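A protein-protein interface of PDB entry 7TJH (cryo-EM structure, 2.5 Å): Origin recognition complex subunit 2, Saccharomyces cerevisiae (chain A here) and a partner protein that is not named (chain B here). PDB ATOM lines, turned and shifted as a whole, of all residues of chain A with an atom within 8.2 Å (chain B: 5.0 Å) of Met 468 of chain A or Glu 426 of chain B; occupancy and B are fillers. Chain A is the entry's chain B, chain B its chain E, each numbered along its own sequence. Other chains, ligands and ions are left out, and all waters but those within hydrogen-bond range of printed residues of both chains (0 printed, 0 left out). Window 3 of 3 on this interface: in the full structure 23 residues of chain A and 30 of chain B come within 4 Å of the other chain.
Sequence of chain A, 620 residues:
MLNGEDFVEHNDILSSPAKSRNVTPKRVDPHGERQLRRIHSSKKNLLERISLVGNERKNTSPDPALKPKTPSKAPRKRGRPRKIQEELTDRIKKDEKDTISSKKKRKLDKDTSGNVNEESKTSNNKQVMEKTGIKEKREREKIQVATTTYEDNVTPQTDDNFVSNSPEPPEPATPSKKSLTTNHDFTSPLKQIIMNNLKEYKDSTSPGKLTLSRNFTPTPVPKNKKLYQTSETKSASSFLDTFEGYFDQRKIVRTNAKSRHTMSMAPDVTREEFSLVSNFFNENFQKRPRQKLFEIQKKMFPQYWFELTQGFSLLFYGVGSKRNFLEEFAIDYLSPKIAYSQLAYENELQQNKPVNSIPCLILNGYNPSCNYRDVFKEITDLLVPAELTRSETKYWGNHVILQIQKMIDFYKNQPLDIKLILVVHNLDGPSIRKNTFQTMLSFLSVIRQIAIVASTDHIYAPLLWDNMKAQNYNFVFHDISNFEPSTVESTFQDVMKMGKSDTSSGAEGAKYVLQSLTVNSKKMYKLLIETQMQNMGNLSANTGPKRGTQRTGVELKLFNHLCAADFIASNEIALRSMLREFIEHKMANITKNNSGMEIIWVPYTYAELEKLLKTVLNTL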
ATOM      1  N   THR A 439     -17.164 -21.689  -3.907  1.00  0.00           N
ATOM      2  CA  THR A 439     -16.162 -20.899  -4.620  1.00  0.00           C
ATOM      3  C   THR A 439     -15.494 -19.896  -3.691  1.00  0.00           C
ATOM      4  O   THR A 439     -14.263 -19.744  -3.706  1.00  0.00           O
ATOM      5  CB  THR A 439     -16.813 -20.176  -5.799  1.00  0.00           C
ATOM      6  OG1 THR A 439     -17.659 -21.083  -6.514  1.00  0.00           O
ATOM      7  CG2 THR A 439     -15.757 -19.618  -6.739  1.00  0.00           C
ATOM      8  N   SER A 442     -13.222 -21.970  -1.154  1.00  0.00           N
ATOM      9  CA  SER A 442     -12.017 -22.509  -1.778  1.00  0.00           C
ATOM     10  C   SER A 442     -11.026 -21.399  -2.113  1.00  0.00           C
ATOM     11  O   SER A 442      -9.810 -21.564  -1.913  1.00  0.00           O
ATOM     12  CB  SER A 442     -12.387 -23.316  -3.021  1.00  0.00           C
ATOM     13  OG  SER A 442     -13.244 -22.585  -3.880  1.00  0.00           O
ATOM     14  N   PHE A 443     -11.525 -20.247  -2.581  1.00  0.00           N
ATOM     15  CA  PHE A 443     -10.641 -19.110  -2.821  1.00  0.00           C
ATOM     16  C   PHE A 443     -10.061 -18.552  -1.522  1.00  0.00           C
ATOM     17  O   PHE A 443      -8.930 -18.056  -1.517  1.00  0.00           O
ATOM     18  CB  PHE A 443     -11.384 -18.023  -3.594  1.00  0.00           C
ATOM     19  CG  PHE A 443     -11.489 -18.283  -5.073  1.00  0.00           C
ATOM     20  CD1 PHE A 443     -10.718 -19.260  -5.684  1.00  0.00           C
ATOM     21  CD2 PHE A 443     -12.355 -17.535  -5.855  1.00  0.00           C
ATOM     22  CE1 PHE A 443     -10.819 -19.491  -7.045  1.00  0.00           C
ATOM     23  CE2 PHE A 443     -12.460 -17.760  -7.216  1.00  0.00           C
ATOM     24  CZ  PHE A 443     -11.691 -18.739  -7.810  1.00  0.00           C
ATOM     25  N   VAL A 446      -7.160 -20.805  -0.625  1.00  0.00           N
ATOM     26  CA  VAL A 446      -5.916 -20.531  -1.354  1.00  0.00           C
ATOM     27  C   VAL A 446      -4.919 -19.776  -0.476  1.00  0.00           C
ATOM     28  O   VAL A 446      -3.709 -20.040  -0.515  1.00  0.00           O
ATOM     29  CB  VAL A 446      -6.228 -19.762  -2.655  1.00  0.00           C
ATOM     30  CG1 VAL A 446      -4.961 -19.415  -3.425  1.00  0.00           C
ATOM     31  CG2 VAL A 446      -7.145 -20.572  -3.535  1.00  0.00           C
ATOM     32  N   PRO A 462     -17.704 -35.387  -1.473  1.00  0.00           N
ATOM     33  CA  PRO A 462     -16.685 -35.095  -2.506  1.00  0.00           C
ATOM     34  C   PRO A 462     -17.224 -34.813  -3.912  1.00  0.00           C
ATOM     35  O   PRO A 462     -16.438 -34.388  -4.768  1.00  0.00           O
ATOM     36  CB  PRO A 462     -15.802 -36.351  -2.506  1.00  0.00           C
ATOM     37  CG  PRO A 462     -16.554 -37.371  -1.760  1.00  0.00           C
ATOM     38  CD  PRO A 462     -17.318 -36.616  -0.747  1.00  0.00           C
ATOM     39  N   LEU A 463     -18.516 -35.013  -4.180  1.00  0.00           N
ATOM     40  CA  LEU A 463     -19.113 -34.543  -5.424  1.00  0.00           C
ATOM     41  C   LEU A 463     -19.206 -33.020  -5.497  1.00  0.00           C
ATOM     42  O   LEU A 463     -19.409 -32.481  -6.590  1.00  0.00           O
ATOM     43  CB  LEU A 463     -20.498 -35.181  -5.596  1.00  0.00           C
ATOM     44  CG  LEU A 463     -21.291 -35.103  -6.904  1.00  0.00           C
ATOM     45  CD1 LEU A 463     -20.515 -35.719  -8.050  1.00  0.00           C
ATOM     46  CD2 LEU A 463     -22.640 -35.778  -6.736  1.00  0.00           C
ATOM     47  N   LEU A 464     -19.035 -32.310  -4.377  1.00  0.00           N
ATOM     48  CA  LEU A 464     -19.078 -30.853  -4.411  1.00  0.00           C
ATOM     49  C   LEU A 464     -17.865 -30.228  -5.097  1.00  0.00           C
ATOM     50  O   LEU A 464     -17.956 -29.081  -5.545  1.00  0.00           O
ATOM     51  CB  LEU A 464     -19.193 -30.293  -2.994  1.00  0.00           C
ATOM     52  CG  LEU A 464     -20.458 -30.620  -2.201  1.00  0.00           C
ATOM     53  CD1 LEU A 464     -20.386 -29.987  -0.826  1.00  0.00           C
ATOM     54  CD2 LEU A 464     -21.705 -30.169  -2.945  1.00  0.00           C
ATOM     55  N   TRP A 465     -16.742 -30.935  -5.190  1.00  0.00           N
ATOM     56  CA  TRP A 465     -15.472 -30.326  -5.574  1.00  0.00           C
ATOM     57  C   TRP A 465     -14.944 -30.943  -6.861  1.00  0.00           C
ATOM     58  O   TRP A 465     -14.725 -32.156  -6.930  1.00  0.00           O
ATOM     59  CB  TRP A 465     -14.442 -30.467  -4.450  1.00  0.00           C
ATOM     60  CG  TRP A 465     -15.018 -30.218  -3.086  1.00  0.00           C
ATOM     61  CD1 TRP A 465     -15.694 -29.108  -2.676  1.00  0.00           C
ATOM     62  CD2 TRP A 465     -14.969 -31.097  -1.958  1.00  0.00           C
ATOM     63  NE1 TRP A 465     -16.071 -29.241  -1.366  1.00  0.00           N
ATOM     64  CE2 TRP A 465     -15.640 -30.454  -0.901  1.00  0.00           C
ATOM     65  CE3 TRP A 465     -14.426 -32.366  -1.739  1.00  0.00           C
ATOM     66  CZ2 TRP A 465     -15.780 -31.036   0.357  1.00  0.00           C
ATOM     67  CZ3 TRP A 465     -14.569 -32.943  -0.490  1.00  0.00           C
ATOM     68  CH2 TRP A 465     -15.239 -32.279   0.541  1.00  0.00           C
ATOM     69  N   ASP A 466     -14.724 -30.099  -7.867  1.00  0.00           N
ATOM     70  CA  ASP A 466     -14.047 -30.475  -9.099  1.00  0.00           C
ATOM     71  C   ASP A 466     -12.537 -30.291  -8.919  1.00  0.00           C
ATOM     72  O   ASP A 466     -12.048 -30.129  -7.801  1.00  0.00           O
ATOM     73  CB  ASP A 466     -14.597 -29.667 -10.275  1.00  0.00           C
ATOM     74  CG  ASP A 466     -14.210 -28.199 -10.216  1.00  0.00           C
ATOM     75  OD1 ASP A 466     -14.163 -27.633  -9.106  1.00  0.00           O
ATOM     76  OD2 ASP A 466     -13.963 -27.608 -11.286  1.00  0.00           O
ATOM     77  N   ASN A 467     -11.786 -30.319 -10.026  1.00  0.00           N
ATOM     78  CA  ASN A 467     -10.328 -30.245  -9.959  1.00  0.00           C
ATOM     79  C   ASN A 467      -9.849 -28.872  -9.499  1.00  0.00           C
ATOM     80  O   ASN A 467      -8.888 -28.779  -8.726  1.00  0.00           O
ATOM     81  CB  ASN A 467      -9.718 -30.594 -11.315  1.00  0.00           C
ATOM     82  CG  ASN A 467      -9.673 -32.086 -11.567  1.00  0.00           C
ATOM     83  OD1 ASN A 467     -10.130 -32.880 -10.745  1.00  0.00           O
ATOM     84  ND2 ASN A 467      -9.133 -32.475 -12.713  1.00  0.00           N
ATOM     85  N   MET A 468     -10.503 -27.803  -9.967  1.00  0.00           N
ATOM     86  CA  MET A 468     -10.190 -26.452  -9.499  1.00  0.00           C
ATOM     87  C   MET A 468     -10.458 -26.307  -8.005  1.00  0.00           C
ATOM     88  O   MET A 468      -9.618 -25.789  -7.260  1.00  0.00           O
ATOM     89  CB  MET A 468     -11.011 -25.423 -10.277  1.00  0.00           C
ATOM     90  CG  MET A 468     -10.425 -24.014 -10.298  1.00  0.00           C
ATOM     91  SD  MET A 468      -8.648 -23.879 -10.560  1.00  0.00           S
ATOM     92  CE  MET A 468      -8.577 -24.044 -12.338  1.00  0.00           C
ATOM     93  N   LYS A 469     -11.609 -26.802  -7.546  1.00  0.00           N
ATOM     94  CA  LYS A 469     -11.978 -26.643  -6.144  1.00  0.00           C
ATOM     95  C   LYS A 469     -11.162 -27.559  -5.240  1.00  0.00           C
ATOM     96  O   LYS A 469     -10.801 -27.164  -4.128  1.00  0.00           O
ATOM     97  CB  LYS A 469     -13.474 -26.887  -5.962  1.00  0.00           C
ATOM     98  CG  LYS A 469     -14.288 -25.607  -5.959  1.00  0.00           C
ATOM     99  CD  LYS A 469     -15.777 -25.878  -5.986  1.00  0.00           C
ATOM    100  CE  LYS A 469     -16.544 -24.634  -6.386  1.00  0.00           C
ATOM    101  NZ  LYS A 469     -17.617 -24.943  -7.364  1.00  0.00           N
ATOM    102  N   ALA A 470     -10.852 -28.778  -5.693  1.00  0.00           N
ATOM    103  CA  ALA A 470     -10.005 -29.653  -4.887  1.00  0.00           C
ATOM    104  C   ALA A 470      -8.566 -29.157  -4.841  1.00  0.00           C
ATOM    105  O   ALA A 470      -7.889 -29.330  -3.822  1.00  0.00           O
ATOM    106  CB  ALA A 470     -10.051 -31.087  -5.415  1.00  0.00           C
ATOM    107  N   GLN A 471      -8.085 -28.548  -5.927  1.00  0.00           N
ATOM    108  CA  GLN A 471      -6.758 -27.945  -5.919  1.00  0.00           C
ATOM    109  C   GLN A 471      -6.696 -26.731  -4.999  1.00  0.00           C
ATOM    110  O   GLN A 471      -5.717 -26.555  -4.266  1.00  0.00           O
ATOM    111  CB  GLN A 471      -6.352 -27.569  -7.342  1.00  0.00           C
ATOM    112  CG  GLN A 471      -4.877 -27.285  -7.517  1.00  0.00           C
ATOM    113  CD  GLN A 471      -4.624 -25.855  -7.943  1.00  0.00           C
ATOM    114  OE1 GLN A 471      -5.544 -25.150  -8.354  1.00  0.00           O
ATOM    115  NE2 GLN A 471      -3.377 -25.415  -7.841  1.00  0.00           N
ATOM    116  N   ASN A 472      -7.729 -25.886  -5.022  1.00  0.00           N
ATOM    117  CA  ASN A 472      -7.728 -24.695  -4.176  1.00  0.00           C
ATOM    118  C   ASN A 472      -7.938 -25.047  -2.709  1.00  0.00           C
ATOM    119  O   ASN A 472      -7.350 -24.413  -1.826  1.00  0.00           O
ATOM    120  CB  ASN A 472      -8.799 -23.718  -4.651  1.00  0.00           C
ATOM    121  CG  ASN A 472      -8.402 -23.000  -5.919  1.00  0.00           C
ATOM    122  OD1 ASN A 472      -7.228 -22.967  -6.283  1.00  0.00           O
ATOM    123  ND2 ASN A 472      -9.380 -22.422  -6.603  1.00  0.00           N
ATOM    124  N   TYR A 473      -8.779 -26.045  -2.432  1.00  0.00           N
ATOM    125  CA  TYR A 473      -9.047 -26.445  -1.055  1.00  0.00           C
ATOM    126  C   TYR A 473      -7.833 -27.108  -0.424  1.00  0.00           C
ATOM    127  O   TYR A 473      -7.493 -26.803   0.726  1.00  0.00           O
ATOM    128  CB  TYR A 473     -10.244 -27.388  -1.007  1.00  0.00           C
ATOM    129  CG  TYR A 473     -11.575 -26.717  -0.762  1.00  0.00           C
ATOM    130  CD1 TYR A 473     -11.737 -25.798   0.270  1.00  0.00           C
ATOM    131  CD2 TYR A 473     -12.679 -27.025  -1.548  1.00  0.00           C
ATOM    132  CE1 TYR A 473     -12.957 -25.198   0.505  1.00  0.00           C
ATOM    133  CE2 TYR A 473     -13.900 -26.429  -1.325  1.00  0.00           C
ATOM    134  CZ  TYR A 473     -14.035 -25.518  -0.300  1.00  0.00           C
ATOM    135  OH  TYR A 473     -15.254 -24.926  -0.083  1.00  0.00           O
ATOM    136  N   ASN A 474      -7.171 -28.006  -1.168  1.00  0.00           N
ATOM    137  CA  ASN A 474      -5.941 -28.702  -0.767  1.00  0.00           C
ATOM    138  C   ASN A 474      -6.142 -29.478   0.540  1.00  0.00           C
ATOM    139  O   ASN A 474      -5.526 -29.203   1.570  1.00  0.00           O
ATOM    140  CB  ASN A 474      -4.768 -27.716  -0.682  1.00  0.00           C
ATOM    141  CG  ASN A 474      -3.428 -28.401  -0.620  1.00  0.00           C
ATOM    142  OD1 ASN A 474      -3.172 -29.365  -1.339  1.00  0.00           O
ATOM    143  ND2 ASN A 474      -2.556 -27.897   0.240  1.00  0.00           N
ATOM    144  N   GLN B 422     -14.495 -36.703  -7.641  1.00  0.00           N
ATOM    145  CA  GLN B 422     -13.867 -35.521  -8.224  1.00  0.00           C
ATOM    146  C   GLN B 422     -13.934 -35.546  -9.750  1.00  0.00           C
ATOM    147  O   GLN B 422     -14.188 -34.513 -10.384  1.00  0.00           O
ATOM    148  CB  GLN B 422     -12.421 -35.418  -7.739  1.00  0.00           C
ATOM    149  CG  GLN B 422     -11.751 -34.086  -8.013  1.00  0.00           C
ATOM    150  CD  GLN B 422     -10.304 -34.070  -7.570  1.00  0.00           C
ATOM    151  OE1 GLN B 422      -9.982 -34.461  -6.449  1.00  0.00           O
ATOM    152  NE2 GLN B 422      -9.420 -33.619  -8.451  1.00  0.00           N
ATOM    153  N   ASN B 423     -13.715 -36.721 -10.354  1.00  0.00           N
ATOM    154  CA  ASN B 423     -13.842 -36.862 -11.804  1.00  0.00           C
ATOM    155  C   ASN B 423     -15.279 -36.646 -12.261  1.00  0.00           C
ATOM    156  O   ASN B 423     -15.516 -36.034 -13.307  1.00  0.00           O
ATOM    157  CB  ASN B 423     -13.347 -38.238 -12.248  1.00  0.00           C
ATOM    158  CG  ASN B 423     -11.842 -38.302 -12.377  1.00  0.00           C
ATOM    159  OD1 ASN B 423     -11.254 -37.665 -13.246  1.00  0.00           O
ATOM    160  ND2 ASN B 423     -11.209 -39.077 -11.507  1.00  0.00           N
ATOM    161  N   LEU B 424     -16.244 -37.141 -11.483  1.00  0.00           N
ATOM    162  CA  LEU B 424     -17.655 -36.928 -11.795  1.00  0.00           C
ATOM    163  C   LEU B 424     -18.030 -35.451 -11.702  1.00  0.00           C
ATOM    164  O   LEU B 424     -18.787 -34.937 -12.542  1.00  0.00           O
ATOM    165  CB  LEU B 424     -18.514 -37.772 -10.855  1.00  0.00           C
ATOM    166  CG  LEU B 424     -20.018 -37.843 -11.110  1.00  0.00           C
ATOM    167  CD1 LEU B 424     -20.307 -38.169 -12.563  1.00  0.00           C
ATOM    168  CD2 LEU B 424     -20.655 -38.862 -10.180  1.00  0.00           C
ATOM    169  N   SER B 425     -17.499 -34.750 -10.695  1.00  0.00           N
ATOM    170  CA  SER B 425     -17.753 -33.319 -10.553  1.00  0.00           C
ATOM    171  C   SER B 425     -17.145 -32.525 -11.707  1.00  0.00           C
ATOM    172  O   SER B 425     -17.771 -31.584 -12.214  1.00  0.00           O
ATOM    173  CB  SER B 425     -17.213 -32.830  -9.207  1.00  0.00           C
ATOM    174  OG  SER B 425     -17.406 -31.436  -9.054  1.00  0.00           O
ATOM    175  N   GLU B 426     -15.934 -32.897 -12.142  1.00  0.00           N
ATOM    176  CA  GLU B 426     -15.338 -32.261 -13.316  1.00  0.00           C
ATOM    177  C   GLU B 426     -16.123 -32.566 -14.584  1.00  0.00           C
ATOM    178  O   GLU B 426     -16.226 -31.715 -15.473  1.00  0.00           O
ATOM    179  CB  GLU B 426     -13.888 -32.697 -13.491  1.00  0.00           C
ATOM    180  CG  GLU B 426     -12.921 -31.769 -12.824  1.00  0.00           C
ATOM    181  CD  GLU B 426     -12.614 -30.555 -13.678  1.00  0.00           C
ATOM    182  OE1 GLU B 426     -12.798 -30.639 -14.910  1.00  0.00           O
ATOM    183  OE2 GLU B 426     -12.217 -29.514 -13.117  1.00  0.00           O
ATOM    184  N   LEU B 427     -16.664 -33.780 -14.685  1.00  0.00           N
ATOM    185  CA  LEU B 427     -17.462 -34.162 -15.841  1.00  0.00           C
ATOM    186  C   LEU B 427     -18.749 -33.351 -15.907  1.00  0.00           C
ATOM    187  O   LEU B 427     -19.222 -33.008 -16.997  1.00  0.00           O
ATOM    188  CB  LEU B 427     -17.751 -35.659 -15.774  1.00  0.00           C
ATOM    189  CG  LEU B 427     -17.463 -36.525 -16.996  1.00  0.00           C
ATOM    190  CD1 LEU B 427     -16.106 -36.195 -17.592  1.00  0.00           C
ATOM    191  CD2 LEU B 427     -17.505 -37.978 -16.575  1.00  0.00           C
ATOM    192  N   HIS B 428     -19.326 -33.031 -14.745  1.00  0.00           N
ATOM    193  CA  HIS B 428     -20.461 -32.113 -14.735  1.00  0.00           C
ATOM    194  C   HIS B 428     -20.028 -30.684 -15.050  1.00  0.00           C
ATOM    195  O   HIS B 428     -20.808 -29.923 -15.636  1.00  0.00           O
ATOM    196  CB  HIS B 428     -21.189 -32.172 -13.391  1.00  0.00           C
ATOM    197  CG  HIS B 428     -22.396 -31.287 -13.317  1.00  0.00           C
ATOM    198  ND1 HIS B 428     -22.322 -29.934 -13.066  1.00  0.00           N
ATOM    199  CD2 HIS B 428     -23.711 -31.564 -13.484  1.00  0.00           C
ATOM    200  CE1 HIS B 428     -23.537 -29.417 -13.080  1.00  0.00           C
ATOM    201  NE2 HIS B 428     -24.398 -30.387 -13.326  1.00  0.00           N
ATOM    202  N   THR B 429     -18.810 -30.297 -14.653  1.00  0.00           N
ATOM    203  CA  THR B 429     -18.314 -28.947 -14.930  1.00  0.00           C
ATOM    204  C   THR B 429     -18.137 -28.710 -16.430  1.00  0.00           C
ATOM    205  O   THR B 429     -18.476 -27.636 -16.943  1.00  0.00           O
ATOM    206  CB  THR B 429     -17.000 -28.718 -14.175  1.00  0.00           C
ATOM    207  OG1 THR B 429     -17.239 -28.809 -12.766  1.00  0.00           O
ATOM    208  CG2 THR B 429     -16.400 -27.355 -14.481  1.00  0.00           C
ATOM    209  N   LEU B 430     -17.660 -29.719 -17.156  1.00  0.00           N
ATOM    210  CA  LEU B 430     -17.429 -29.630 -18.595  1.00  0.00           C
ATOM    211  C   LEU B 430     -18.700 -29.803 -19.425  1.00  0.00           C
ATOM    212  O   LEU B 430     -18.622 -29.722 -20.655  1.00  0.00           O
ATOM    213  CB  LEU B 430     -16.393 -30.679 -19.010  1.00  0.00           C
ATOM    214  CG  LEU B 430     -15.026 -30.559 -18.333  1.00  0.00           C
ATOM    215  CD1 LEU B 430     -14.095 -31.684 -18.759  1.00  0.00           C
ATOM    216  CD2 LEU B 430     -14.396 -29.204 -18.607  1.00  0.00           C
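Among the printed residues, pairs that only touch across the chains: Ala 470 of chain A with Gln 422 of chain B (3.5 Å), Trp 465 of chain A with Gln 422 of chain B (3.7 Å), Asp 466 of chain A with Thr 429 of chain B (3.7 Å), Leu 463 of chain A with Leu 424 of chain B (3.8 Å), Met 468 of chain A with Glu 426 of chain B (3.97 Å) and Asp 466 of chain A with Gln 422 of chain B (3.97 Å).
Of the 17 printed residues of chain A, 6 touch a printed residue of chain B. Of the 9 printed residues of chain B, 5 touch a printed residue of chain A. Among the printed residues, no Asp or Glu carboxylate lies within 4 Å of a Lys or Arg side-chain nitrogen of the other chain.
Glu 426 of chain B touches just these residues of chain A: Asp 466, Asn 467 and Met 468. Of the printed residues of chain A, Ser 425 of chain B touches Leu 463 (3.3 Å), Trp 465 (3.3 Å) and Asp 466 (3.2 Å). Printed residues of chain A within 4 Å of Leu 424 of chain B: Leu 463 (3.8 Å). Of the printed residues of chain B, Asn 467 of chain A touches Gln 422 and Glu 426. The nearest residue of chain A that does not touch Glu 426 of chain B is Trp 465 of chain A (5.4 Å). The nearest printed residue of chain B that does not touch Asn 467 of chain A is Asn 423 of chain B (5.3 Å).
The side-chain carboxylate (OD1) of Asp 466 of chain A sits at hydrogen-bond distance from the backbone NH (N) of Lys 469 of chain A (3.1 Å). ND2 of Asn 472 of chain A sits close to O of Met 468 of chain A (3.4 Å). The backbone carbonyl oxygen of Ser 425 of chain B lies within hydrogen-bond range of the side-chain hydroxyl of Thr 429 of chain B.
The backbone carbonyl oxygen of Leu 463 of chain A sits at hydrogen-bond distance from the side-chain hydroxyl of Ser 425 of chain B (3.3 Å). The side-chain hydroxyl (OG) of Ser 425 of chain B sits close to the backbone carbonyl oxygen (O) of Trp 465 of chain A, 3.5 Å away. The side-chain hydroxyl (OG) of Ser 425 of chain B lies within hydrogen-bond range of the backbone NH (N) of Asp 466 of chain A (3.2 Å). The side-chain amide oxygen of Asn 467 of chain A is in hydrogen-bond range of the side-chain amide nitrogen of Gln 422 of chain B, at 2.5 Å. The side-chain carboxylate of Glu 426 of chain B is in hydrogen-bond range of the backbone NH of Asn 467 of chain A, 3.2 Å away. OE2 of Glu 426 of chain B sits close to OD2 of Asp 466 of chain A (3.2 Å).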
